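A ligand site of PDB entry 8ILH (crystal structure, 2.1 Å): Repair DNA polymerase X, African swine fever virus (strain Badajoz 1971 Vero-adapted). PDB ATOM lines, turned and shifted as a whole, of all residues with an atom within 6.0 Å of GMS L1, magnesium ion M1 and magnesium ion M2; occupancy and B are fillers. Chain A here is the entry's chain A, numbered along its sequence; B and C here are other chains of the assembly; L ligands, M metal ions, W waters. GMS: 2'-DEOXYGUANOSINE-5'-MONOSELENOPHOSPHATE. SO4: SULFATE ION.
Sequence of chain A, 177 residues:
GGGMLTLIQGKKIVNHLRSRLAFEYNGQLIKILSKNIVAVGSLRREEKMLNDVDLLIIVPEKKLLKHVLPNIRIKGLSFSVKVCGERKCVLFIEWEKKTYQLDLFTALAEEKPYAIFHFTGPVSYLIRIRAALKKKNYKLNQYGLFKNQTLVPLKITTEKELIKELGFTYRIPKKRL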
ATOM      1  N   VAL A  40      18.985 -28.327  -1.251  1.00  0.00           N
ATOM      2  CA  VAL A  40      18.920 -27.006  -0.619  1.00  0.00           C
ATOM      3  C   VAL A  40      20.107 -26.889   0.358  1.00  0.00           C
ATOM      4  O   VAL A  40      21.062 -27.649   0.244  1.00  0.00           O
ATOM      5  CB  VAL A  40      17.535 -26.772   0.056  1.00  0.00           C
ATOM      6  CG1 VAL A  40      16.450 -26.694  -1.010  1.00  0.00           C
ATOM      7  CG2 VAL A  40      17.220 -27.870   1.065  1.00  0.00           C
ATOM      8  N   GLY A  41      20.073 -25.916   1.266  1.00  0.00           N
ATOM      9  CA  GLY A  41      21.138 -25.742   2.245  1.00  0.00           C
ATOM     10  C   GLY A  41      22.492 -25.399   1.647  1.00  0.00           C
ATOM     11  O   GLY A  41      22.584 -24.903   0.510  1.00  0.00           O
ATOM     12  N   SER A  42      23.548 -25.682   2.398  1.00  0.00           N
ATOM     13  CA  SER A  42      24.914 -25.316   1.980  1.00  0.00           C
ATOM     14  C   SER A  42      25.363 -26.036   0.700  1.00  0.00           C
ATOM     15  O   SER A  42      26.167 -25.494  -0.063  1.00  0.00           O
ATOM     16  CB  SER A  42      25.923 -25.539   3.120  1.00  0.00           C
ATOM     17  OG  SER A  42      25.954 -26.884   3.528  1.00  0.00           O
ATOM     18  N   LEU A  43      24.799 -27.226   0.452  1.00  0.00           N
ATOM     19  CA  LEU A  43      25.036 -27.968  -0.787  1.00  0.00           C
ATOM     20  C   LEU A  43      24.603 -27.173  -2.011  1.00  0.00           C
ATOM     21  O   LEU A  43      25.361 -27.077  -2.968  1.00  0.00           O
ATOM     22  CB  LEU A  43      24.270 -29.290  -0.766  1.00  0.00           C
ATOM     23  CG  LEU A  43      24.286 -30.321  -1.890  1.00  0.00           C
ATOM     24  CD1 LEU A  43      25.639 -30.500  -2.486  1.00  0.00           C
ATOM     25  CD2 LEU A  43      23.788 -31.698  -1.432  1.00  0.00           C
ATOM     26  N   ARG A  45      24.264 -23.960  -2.039  1.00  0.00           N
ATOM     27  CA  ARG A  45      25.165 -22.796  -2.019  1.00  0.00           C
ATOM     28  C   ARG A  45      26.611 -23.125  -2.443  1.00  0.00           C
ATOM     29  O   ARG A  45      27.435 -22.226  -2.524  1.00  0.00           O
ATOM     30  CB  ARG A  45      25.150 -22.127  -0.635  1.00  0.00           C
ATOM     31  CG  ARG A  45      23.799 -21.529  -0.267  1.00  0.00           C
ATOM     32  CD  ARG A  45      23.902 -20.512   0.869  1.00  0.00           C
ATOM     33  NE  ARG A  45      24.734 -20.983   1.977  1.00  0.00           N
ATOM     34  CZ  ARG A  45      24.336 -21.770   2.995  1.00  0.00           C
ATOM     35  NH1 ARG A  45      23.083 -22.222   3.086  1.00  0.00           N
ATOM     36  NH2 ARG A  45      25.212 -22.118   3.936  1.00  0.00           N
ATOM     37  N   ASN A  51      28.220 -29.659   6.632  1.00  0.00           N
ATOM     38  CA  ASN A  51      27.880 -30.301   7.915  1.00  0.00           C
ATOM     39  C   ASN A  51      26.832 -31.406   7.742  1.00  0.00           C
ATOM     40  O   ASN A  51      26.751 -32.316   8.569  1.00  0.00           O
ATOM     41  CB  ASN A  51      27.467 -29.271   8.972  1.00  0.00           C
ATOM     42  CG  ASN A  51      28.654 -28.469   9.485  1.00  0.00           C
ATOM     43  OD1 ASN A  51      29.681 -29.042   9.869  1.00  0.00           O
ATOM     44  ND2 ASN A  51      28.535 -27.148   9.488  1.00  0.00           N
ATOM     45  N   ASP A  52      26.121 -31.373   6.622  1.00  0.00           N
ATOM     46  CA  ASP A  52      25.115 -32.379   6.277  1.00  0.00           C
ATOM     47  C   ASP A  52      24.558 -32.183   4.886  1.00  0.00           C
ATOM     48  O   ASP A  52      24.969 -31.330   4.194  1.00  0.00           O
ATOM     49  CB  ASP A  52      23.969 -32.292   7.238  1.00  0.00           C
ATOM     50  CG  ASP A  52      23.560 -30.901   7.514  1.00  0.00           C
ATOM     51  OD1 ASP A  52      23.047 -30.271   6.648  1.00  0.00           O
ATOM     52  OD2 ASP A  52      23.860 -30.398   8.562  1.00  0.00           O
ATOM     53  N   VAL A  53      23.612 -33.010   4.494  1.00  0.00           N
ATOM     54  CA  VAL A  53      22.924 -32.877   3.213  1.00  0.00           C
ATOM     55  C   VAL A  53      21.463 -32.506   3.490  1.00  0.00           C
ATOM     56  O   VAL A  53      20.789 -33.173   4.276  1.00  0.00           O
ATOM     57  CB  VAL A  53      22.979 -34.197   2.406  1.00  0.00           C
ATOM     58  CG1 VAL A  53      22.223 -34.076   1.085  1.00  0.00           C
ATOM     59  CG2 VAL A  53      24.420 -34.569   2.141  1.00  0.00           C
ATOM     60  N   ASP A  54      21.001 -31.462   2.814  1.00  0.00           N
ATOM     61  CA  ASP A  54      19.620 -30.974   2.962  1.00  0.00           C
ATOM     62  C   ASP A  54      18.831 -31.202   1.691  1.00  0.00           C
ATOM     63  O   ASP A  54      19.250 -30.745   0.624  1.00  0.00           O
ATOM     64  CB  ASP A  54      19.621 -29.478   3.280  1.00  0.00           C
ATOM     65  CG  ASP A  54      20.399 -29.161   4.523  1.00  0.00           C
ATOM     66  OD1 ASP A  54      20.037 -29.678   5.593  1.00  0.00           O
ATOM     67  OD2 ASP A  54      21.363 -28.367   4.441  1.00  0.00           O
ATOM     68  N   GLN A 101      24.731 -36.928   8.355  1.00  0.00           N
ATOM     69  CA  GLN A 101      23.406 -36.409   8.618  1.00  0.00           C
ATOM     70  C   GLN A 101      22.698 -35.997   7.326  1.00  0.00           C
ATOM     71  O   GLN A 101      23.269 -35.237   6.522  1.00  0.00           O
ATOM     72  CB  GLN A 101      23.491 -35.220   9.565  1.00  0.00           C
ATOM     73  CG  GLN A 101      22.140 -34.684   9.972  1.00  0.00           C
ATOM     74  CD  GLN A 101      22.180 -33.756  11.171  1.00  0.00           C
ATOM     75  OE1 GLN A 101      22.865 -34.033  12.165  1.00  0.00           O
ATOM     76  NE2 GLN A 101      21.451 -32.637  11.089  1.00  0.00           N
ATOM     77  N   ASP A 103      19.153 -34.222   6.196  1.00  0.00           N
ATOM     78  CA  ASP A 103      17.990 -33.478   6.650  1.00  0.00           C
ATOM     79  C   ASP A 103      16.932 -33.403   5.543  1.00  0.00           C
ATOM     80  O   ASP A 103      17.210 -32.920   4.449  1.00  0.00           O
ATOM     81  CB  ASP A 103      18.389 -32.068   7.091  1.00  0.00           C
ATOM     82  CG  ASP A 103      19.061 -32.056   8.453  1.00  0.00           C
ATOM     83  OD1 ASP A 103      19.110 -33.115   9.103  1.00  0.00           O
ATOM     84  OD2 ASP A 103      19.542 -30.977   8.867  1.00  0.00           O
ATOM     85  N   PHE A 105      13.093 -32.130   4.387  1.00  0.00           N
ATOM     86  CA  PHE A 105      12.012 -31.167   4.637  1.00  0.00           C
ATOM     87  C   PHE A 105      10.932 -31.331   3.593  1.00  0.00           C
ATOM     88  O   PHE A 105      11.220 -31.767   2.474  1.00  0.00           O
ATOM     89  CB  PHE A 105      12.569 -29.743   4.601  1.00  0.00           C
ATOM     90  CG  PHE A 105      13.766 -29.541   5.478  1.00  0.00           C
ATOM     91  CD1 PHE A 105      13.623 -29.348   6.834  1.00  0.00           C
ATOM     92  CD2 PHE A 105      15.042 -29.526   4.928  1.00  0.00           C
ATOM     93  CE1 PHE A 105      14.719 -29.127   7.637  1.00  0.00           C
ATOM     94  CE2 PHE A 105      16.167 -29.300   5.736  1.00  0.00           C
ATOM     95  CZ  PHE A 105      16.003 -29.096   7.090  1.00  0.00           C
ATOM     96  N   HIS A 118      13.823 -20.156   1.550  1.00  0.00           N
ATOM     97  CA  HIS A 118      14.125 -20.363   2.971  1.00  0.00           C
ATOM     98  C   HIS A 118      15.236 -21.382   3.199  1.00  0.00           C
ATOM     99  O   HIS A 118      16.233 -21.085   3.851  1.00  0.00           O
ATOM    100  CB  HIS A 118      12.855 -20.780   3.739  1.00  0.00           C
ATOM    101  CG  HIS A 118      13.115 -21.286   5.131  1.00  0.00           C
ATOM    102  ND1 HIS A 118      12.996 -20.498   6.248  1.00  0.00           N
ATOM    103  CD2 HIS A 118      13.418 -22.513   5.580  1.00  0.00           C
ATOM    104  CE1 HIS A 118      13.260 -21.201   7.336  1.00  0.00           C
ATOM    105  NE2 HIS A 118      13.524 -22.434   6.954  1.00  0.00           N
ATOM    106  N   PHE A 119      15.064 -22.592   2.650  1.00  0.00           N
ATOM    107  CA  PHE A 119      16.029 -23.686   2.904  1.00  0.00           C
ATOM    108  C   PHE A 119      17.369 -23.525   2.193  1.00  0.00           C
ATOM    109  O   PHE A 119      18.306 -24.214   2.530  1.00  0.00           O
ATOM    110  CB  PHE A 119      15.403 -25.057   2.608  1.00  0.00           C
ATOM    111  CG  PHE A 119      14.368 -25.454   3.599  1.00  0.00           C
ATOM    112  CD1 PHE A 119      14.734 -25.795   4.881  1.00  0.00           C
ATOM    113  CD2 PHE A 119      13.013 -25.457   3.265  1.00  0.00           C
ATOM    114  CE1 PHE A 119      13.779 -26.153   5.824  1.00  0.00           C
ATOM    115  CE2 PHE A 119      12.060 -25.813   4.194  1.00  0.00           C
ATOM    116  CZ  PHE A 119      12.443 -26.155   5.478  1.00  0.00           C
ATOM    117  N   THR A 120      17.466 -22.604   1.233  1.00  0.00           N
ATOM    118  CA  THR A 120      18.749 -22.278   0.623  1.00  0.00           C
ATOM    119  C   THR A 120      19.624 -21.445   1.565  1.00  0.00           C
ATOM    120  O   THR A 120      20.838 -21.642   1.591  1.00  0.00           O
ATOM    121  CB  THR A 120      18.549 -21.547  -0.705  1.00  0.00           C
ATOM    122  OG1 THR A 120      17.891 -22.445  -1.609  1.00  0.00           O
ATOM    123  CG2 THR A 120      19.897 -21.125  -1.319  1.00  0.00           C
ATOM    124  N   GLY A 121      19.012 -20.545   2.335  1.00  0.00           N
ATOM    125  CA  GLY A 121      19.773 -19.681   3.231  1.00  0.00           C
ATOM    126  C   GLY A 121      20.740 -18.810   2.439  1.00  0.00           C
ATOM    127  O   GLY A 121      20.443 -18.445   1.300  1.00  0.00           O
ATOM    128  N   PRO A 122      21.882 -18.447   3.020  1.00  0.00           N
ATOM    129  CA  PRO A 122      22.266 -18.741   4.399  1.00  0.00           C
ATOM    130  C   PRO A 122      21.433 -17.959   5.409  1.00  0.00           C
ATOM    131  O   PRO A 122      20.700 -17.045   5.044  1.00  0.00           O
ATOM    132  CB  PRO A 122      23.722 -18.269   4.453  1.00  0.00           C
ATOM    133  CG  PRO A 122      23.747 -17.100   3.499  1.00  0.00           C
ATOM    134  CD  PRO A 122      22.792 -17.464   2.392  1.00  0.00           C
ATOM    135  N   VAL A 123      21.593 -18.324   6.682  1.00  0.00           N
ATOM    136  CA  VAL A 123      20.774 -17.761   7.764  1.00  0.00           C
ATOM    137  C   VAL A 123      20.917 -16.239   7.829  1.00  0.00           C
ATOM    138  O   VAL A 123      19.911 -15.514   7.887  1.00  0.00           O
ATOM    139  CB  VAL A 123      21.113 -18.427   9.122  1.00  0.00           C
ATOM    140  CG1 VAL A 123      20.315 -17.788  10.255  1.00  0.00           C
ATOM    141  CG2 VAL A 123      20.781 -19.909   9.068  1.00  0.00           C
ATOM    142  N   LEU A 126      18.798 -14.515   5.179  1.00  0.00           N
ATOM    143  CA  LEU A 126      17.376 -14.579   5.506  1.00  0.00           C
ATOM    144  C   LEU A 126      17.009 -13.548   6.584  1.00  0.00           C
ATOM    145  O   LEU A 126      15.983 -12.873   6.450  1.00  0.00           O
ATOM    146  CB  LEU A 126      16.979 -15.980   5.980  1.00  0.00           C
ATOM    147  CG  LEU A 126      17.149 -17.123   4.994  1.00  0.00           C
ATOM    148  CD1 LEU A 126      16.676 -18.391   5.663  1.00  0.00           C
ATOM    149  CD2 LEU A 126      16.398 -16.897   3.693  1.00  0.00           C
ATOM    150  N   ILE A 127      17.839 -13.434   7.616  1.00  0.00           N
ATOM    151  CA  ILE A 127      17.605 -12.491   8.717  1.00  0.00           C
ATOM    152  C   ILE A 127      17.481 -11.058   8.175  1.00  0.00           C
ATOM    153  O   ILE A 127      16.540 -10.326   8.518  1.00  0.00           O
ATOM    154  CB  ILE A 127      18.708 -12.606   9.794  1.00  0.00           C
ATOM    155  CG1 ILE A 127      18.527 -13.927  10.570  1.00  0.00           C
ATOM    156  CG2 ILE A 127      18.640 -11.440  10.782  1.00  0.00           C
ATOM    157  CD1 ILE A 127      19.619 -14.283  11.559  1.00  0.00           C
ATOM    158  N   ARG A 130      14.337 -10.683   5.920  1.00  0.00           N
ATOM    159  CA  ARG A 130      13.121 -10.748   6.722  1.00  0.00           C
ATOM    160  C   ARG A 130      12.949  -9.489   7.584  1.00  0.00           C
ATOM    161  O   ARG A 130      11.825  -8.993   7.738  1.00  0.00           O
ATOM    162  CB  ARG A 130      13.112 -12.023   7.572  1.00  0.00           C
ATOM    163  CG  ARG A 130      12.867 -13.255   6.713  1.00  0.00           C
ATOM    164  CD  ARG A 130      13.101 -14.574   7.434  1.00  0.00           C
ATOM    165  NE  ARG A 130      12.731 -15.629   6.511  1.00  0.00           N
ATOM    166  CZ  ARG A 130      12.310 -16.855   6.846  1.00  0.00           C
ATOM    167  NH1 ARG A 130      12.220 -17.271   8.107  1.00  0.00           N
ATOM    168  NH2 ARG A 130      12.003 -17.680   5.848  1.00  0.00           N
ATOM    169  P    DC B   7      20.216 -29.623  13.568  1.00  0.00           P
ATOM    170  OP1  DC B   7      20.378 -30.973  13.087  1.00  0.00           O
ATOM    171  OP2  DC B   7      21.400 -28.778  13.661  1.00  0.00           O
ATOM    172  O5'  DC B   7      19.198 -28.772  12.684  1.00  0.00           O
ATOM    173  C5'  DC B   7      18.413 -29.322  11.638  1.00  0.00           C
ATOM    174  C4'  DC B   7      17.659 -28.250  10.871  1.00  0.00           C
ATOM    175  O4'  DC B   7      16.838 -27.472  11.766  1.00  0.00           O
ATOM    176  C3'  DC B   7      18.466 -27.189  10.143  1.00  0.00           C
ATOM    177  O3'  DC B   7      19.216 -27.516   8.972  1.00  0.00           O
ATOM    178  C2'  DC B   7      17.379 -26.184   9.843  1.00  0.00           C
ATOM    179  C1'  DC B   7      16.558 -26.223  11.128  1.00  0.00           C
ATOM    180  N1   DC B   7      16.852 -25.120  12.050  1.00  0.00           N
ATOM    181  C2   DC B   7      16.058 -23.983  11.992  1.00  0.00           C
ATOM    182  O2   DC B   7      15.081 -23.981  11.251  1.00  0.00           O
ATOM    183  N3   DC B   7      16.320 -22.947  12.819  1.00  0.00           N
ATOM    184  C4   DC B   7      17.365 -22.999  13.638  1.00  0.00           C
ATOM    185  N4   DC B   7      17.605 -21.947  14.414  1.00  0.00           N
ATOM    186  C5   DC B   7      18.231 -24.128  13.686  1.00  0.00           C
ATOM    187  C6   DC B   7      17.946 -25.157  12.872  1.00  0.00           C
ATOM    188  O5'  DC C   1      14.814 -10.625  13.188  1.00  0.00           O
ATOM    189  C5'  DC C   1      14.775 -10.486  11.752  1.00  0.00           C
ATOM    190  C4'  DC C   1      13.872 -11.503  11.093  1.00  0.00           C
ATOM    191  O4'  DC C   1      14.576 -12.735  10.797  1.00  0.00           O
ATOM    192  C3'  DC C   1      12.606 -11.893  11.853  1.00  0.00           C
ATOM    193  O3'  DC C   1      11.508 -11.827  10.942  1.00  0.00           O
ATOM    194  C2'  DC C   1      12.905 -13.304  12.363  1.00  0.00           C
ATOM    195  C1'  DC C   1      13.883 -13.860  11.325  1.00  0.00           C
ATOM    196  N1   DC C   1      14.896 -14.792  11.847  1.00  0.00           N
ATOM    197  C2   DC C   1      15.088 -16.028  11.209  1.00  0.00           C
ATOM    198  O2   DC C   1      14.382 -16.321  10.241  1.00  0.00           O
ATOM    199  N3   DC C   1      16.040 -16.873  11.673  1.00  0.00           N
ATOM    200  C4   DC C   1      16.792 -16.515  12.716  1.00  0.00           C
ATOM    201  N4   DC C   1      17.722 -17.381  13.152  1.00  0.00           N
ATOM    202  C5   DC C   1      16.628 -15.266  13.382  1.00  0.00           C
ATOM    203  C6   DC C   1      15.685 -14.439  12.916  1.00  0.00           C
ATOM    204  P    DG C   2      10.009 -12.046  11.441  1.00  0.00           P
ATOM    205  OP1  DG C   2       9.098 -11.446  10.447  1.00  0.00           O
ATOM    206  OP2  DG C   2       9.921 -11.667  12.873  1.00  0.00           O
ATOM    207  O5'  DG C   2       9.831 -13.623  11.376  1.00  0.00           O
ATOM    208  C5'  DG C   2       9.828 -14.292  10.112  1.00  0.00           C
ATOM    209  C4'  DG C   2       9.820 -15.781  10.352  1.00  0.00           C
ATOM    210  O4'  DG C   2      11.108 -16.195  10.871  1.00  0.00           O
ATOM    211  C3'  DG C   2       8.781 -16.288  11.374  1.00  0.00           C
ATOM    212  O3'  DG C   2       7.749 -17.008  10.707  1.00  0.00           O
ATOM    213  C2'  DG C   2       9.604 -17.111  12.361  1.00  0.00           C
ATOM    214  C1'  DG C   2      10.868 -17.369  11.586  1.00  0.00           C
ATOM    215  N9   DG C   2      12.038 -17.662  12.401  1.00  0.00           N
ATOM    216  C8   DG C   2      12.543 -16.914  13.439  1.00  0.00           C
ATOM    217  N7   DG C   2      13.566 -17.486  14.019  1.00  0.00           N
ATOM    218  C5   DG C   2      13.745 -18.678  13.329  1.00  0.00           C
ATOM    219  C6   DG C   2      14.696 -19.713  13.506  1.00  0.00           C
ATOM    220  O6   DG C   2      15.608 -19.786  14.341  1.00  0.00           O
ATOM    221  N1   DG C   2      14.501 -20.750  12.601  1.00  0.00           N
ATOM    222  C2   DG C   2      13.519 -20.785  11.643  1.00  0.00           C
ATOM    223  N2   DG C   2      13.488 -21.867  10.852  1.00  0.00           N
ATOM    224  N3   DG C   2      12.626 -19.821  11.461  1.00  0.00           N
ATOM    225  C4   DG C   2      12.798 -18.806  12.338  1.00  0.00           C
ATOM    226  P    DG C   3       6.633 -17.827  11.518  1.00  0.00           P
ATOM    227  OP1  DG C   3       5.408 -17.878  10.693  1.00  0.00           O
ATOM    228  OP2  DG C   3       6.562 -17.306  12.891  1.00  0.00           O
ATOM    229  O5'  DG C   3       7.282 -19.283  11.617  1.00  0.00           O
ATOM    230  C5'  DG C   3       7.591 -20.022  10.417  1.00  0.00           C
ATOM    231  C4'  DG C   3       8.098 -21.400  10.765  1.00  0.00           C
ATOM    232  O4'  DG C   3       9.370 -21.285  11.448  1.00  0.00           O
ATOM    233  C3'  DG C   3       7.191 -22.248  11.670  1.00  0.00           C
ATOM    234  O3'  DG C   3       7.017 -23.520  11.030  1.00  0.00           O
ATOM    235  C2'  DG C   3       7.954 -22.305  12.981  1.00  0.00           C
ATOM    236  C1'  DG C   3       9.384 -22.210  12.508  1.00  0.00           C
ATOM    237  N9   DG C   3      10.299 -21.721  13.524  1.00  0.00           N
ATOM    238  C8   DG C   3      10.176 -20.560  14.259  1.00  0.00           C
ATOM    239  N7   DG C   3      11.142 -20.396  15.121  1.00  0.00           N
ATOM    240  C5   DG C   3      11.959 -21.506  14.941  1.00  0.00           C
ATOM    241  C6   DG C   3      13.148 -21.887  15.598  1.00  0.00           C
ATOM    242  O6   DG C   3      13.762 -21.291  16.485  1.00  0.00           O
ATOM    243  N1   DG C   3      13.649 -23.088  15.107  1.00  0.00           N
ATOM    244  C2   DG C   3      13.062 -23.844  14.123  1.00  0.00           C
ATOM    245  N2   DG C   3      13.676 -24.985  13.788  1.00  0.00           N
ATOM    246  N3   DG C   3      11.941 -23.497  13.505  1.00  0.00           N
ATOM    247  C4   DG C   3      11.444 -22.337  13.967  1.00  0.00           C
HETATM  248  P   GMS L   1      20.525 -26.638   8.544  1.00  0.00           P
HETATM  249 SE   GMS L   1      21.590 -27.769   7.501  1.00  0.00          SE
HETATM  250  O5' GMS L   1      19.905 -25.566   7.512  1.00  0.00           O
HETATM  251  N9  GMS L   1      17.810 -22.333   8.167  1.00  0.00           N
HETATM  252  C4  GMS L   1      17.224 -21.267   8.818  1.00  0.00           C
HETATM  253  N3  GMS L   1      16.293 -20.439   8.296  1.00  0.00           N
HETATM  254  C2  GMS L   1      15.913 -19.509   9.166  1.00  0.00           C
HETATM  255  N2  GMS L   1      15.003 -18.594   8.814  1.00  0.00           N
HETATM  256  N1  GMS L   1      16.410 -19.416  10.448  1.00  0.00           N
HETATM  257  C6  GMS L   1      17.366 -20.255  10.993  1.00  0.00           C
HETATM  258  O6  GMS L   1      17.745 -20.078  12.160  1.00  0.00           O
HETATM  259  C5  GMS L   1      17.780 -21.253  10.072  1.00  0.00           C
HETATM  260  N7  GMS L   1      18.705 -22.278  10.225  1.00  0.00           N
HETATM  261  C8  GMS L   1      18.697 -22.879   9.067  1.00  0.00           C
HETATM  262  C2' GMS L   1      18.751 -22.247   5.878  1.00  0.00           C
HETATM  263  C5' GMS L   1      19.207 -25.911   6.419  1.00  0.00           C
HETATM  264  C4' GMS L   1      18.700 -24.595   5.894  1.00  0.00           C
HETATM  265  O4' GMS L   1      17.577 -24.143   6.699  1.00  0.00           O
HETATM  266  C1' GMS L   1      17.602 -22.712   6.777  1.00  0.00           C
HETATM  267  C3' GMS L   1      19.693 -23.441   5.967  1.00  0.00           C
HETATM  268  O3' GMS L   1      20.788 -23.537   5.040  1.00  0.00           O
HETATM  269  OP2 GMS L   1      21.191 -26.020   9.840  1.00  0.00           O
HETATM  270  S   SO4 L   2      23.424 -24.760   6.297  1.00  0.00           S
HETATM  271  O1  SO4 L   2      23.240 -23.333   5.927  1.00  0.00           O
HETATM  272  O2  SO4 L   2      24.822 -24.972   6.707  1.00  0.00           O
HETATM  273  O3  SO4 L   2      23.114 -25.614   5.128  1.00  0.00           O
HETATM  274  O4  SO4 L   2      22.517 -25.096   7.410  1.00  0.00           O
HETATM  275 MG    MG M   1      22.990 -28.025   5.905  1.00  0.00          MG
HETATM  276 MG    MG M   2      20.630 -29.599   7.544  1.00  0.00          MG
HETATM  277  O   HOH W   1      21.009 -23.040  11.898  1.00  0.00           O
HETATM  278  O   HOH W   2      24.247 -28.488   4.282  1.00  0.00           O
HETATM  279  O   HOH W   3      20.295 -20.506  13.207  1.00  0.00           O
HETATM  280  O   HOH W   4      24.653 -27.961   7.781  1.00  0.00           O
HETATM  281  O   HOH W   5      14.626 -24.545   8.493  1.00  0.00           O
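Magnesium ion M1 is bound by water W2 (2.1 Å), SE of GMS L1 (2.1 Å), OD2 of Asp 54 (2.2 Å), OD1 of Asp 52 (2.4 Å), water W4 (2.5 Å) and O3 of SO4 L2 (2.5 Å).
Magnesium ion M2 is bound by the side-chain carboxylate of Asp 54 (2.0 Å), a selenium (SE) of GMS L1 (2.1 Å) and the side-chain carboxylate of Asp 103 (2.2 Å). Slightly farther from magnesium ion M2 lies the side-chain carboxylate (OD1) of Asp 52 (2.7 Å).
A phosphorus (P) of GMS L1 is bonded to O3' of DC 7 of chain B, 1.6 Å away. NH1 of Arg 45 lies within hydrogen-bond range of O3' of GMS L1 (3.3 Å). O2 of DC 1 of chain C sits at hydrogen-bond distance from N2 of GMS L1. A nitrogen (N1) of GMS L1 sits at hydrogen-bond distance from N1 of DG 2 of chain C, 3.2 Å away.
Water W2 lies within hydrogen-bond range of OG of Ser 42 (2.5 Å) and O of Asp 52 (2.9 Å). Water W3 bridges an oxygen (O6) of GMS L1 (2.8 Å) and N4 of DC 7 of chain B (3.3 Å). Water W5 lies within hydrogen-bond range of a ring nitrogen (NE2) of His 118 (2.8 Å), O2 of DC 7 of chain B (2.9 Å) and an oxygen (O4') of GMS L1 (3.5 Å).
Merely in contact with magnesium ion M1: Ser 42. Three residues have an atom within 4 Å of magnesium ion M1: Ser 42, Asp 52 and Asp 54. The nearest printed residue that does not touch magnesium ion M1 is Gly 41 (4.7 Å).
N2 of GMS L1 lies close to NH1 of Arg 130 (3.2 Å). Gly 41 touches GMS L1 (CA to O3', 3.6 Å). CE1 of His 118 touches N3 of GMS L1 (3.3 Å). Phe 119 touches GMS L1 (O to C4', 3.4 Å). Thr 120 touches GMS L1. CA of Gly 121 touches C2' of GMS L1, at 3.8 Å. Val 123 touches GMS L1 (CG2 to N7, 3.4 Å). CD1 of Leu 126 touches N3 of GMS L1 (3.4 Å). Hydrophobic or aromatic side chains within 4 Å of GMS L1: His 118, Phe 119, Val 123 and Leu 126. Within 4 Å of GMS L1: Gly 41, Arg 45, Asp 52, Asp 54, His 118, Phe 119, Thr 120, Gly 121, Val 123, Leu 126, Arg 130, DC 7 of chain B, DC 1 of chain C and DG 2 of chain C.
N2 of DG 2 of chain C sits close to O2 of DC 7 of chain B (2.7 Å). N of Val 40 is in hydrogen-bond range of O of Asp 54. NH1 of Arg 45 lies within hydrogen-bond range of O of Thr 120 (2.8 Å). The guanidinium group (NH2) of Arg 130 sits at hydrogen-bond distance from a ring nitrogen (ND1) of His 118 (3.0 Å). O4' of DG 2 of chain C is in hydrogen-bond range of the guanidinium group (NH1) of Arg 130. The backbone carbonyl oxygen (O) of Val 53 lies within hydrogen-bond range of the backbone NH (N) of Asp 103, 2.7 Å away. The guanidinium group of Arg 130 sits at hydrogen-bond distance from O2 of DC 1 of chain C, at 3.2 Å. OD1 of Asp 103 is in hydrogen-bond range of NE2 of Gln 101.
Residues that only touch magnesium ion M2: DC 7 of chain B. Four residues have an atom within 4 Å of magnesium ion M2: Asp 52, Asp 54, Asp 103 and DC 7 of chain B.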
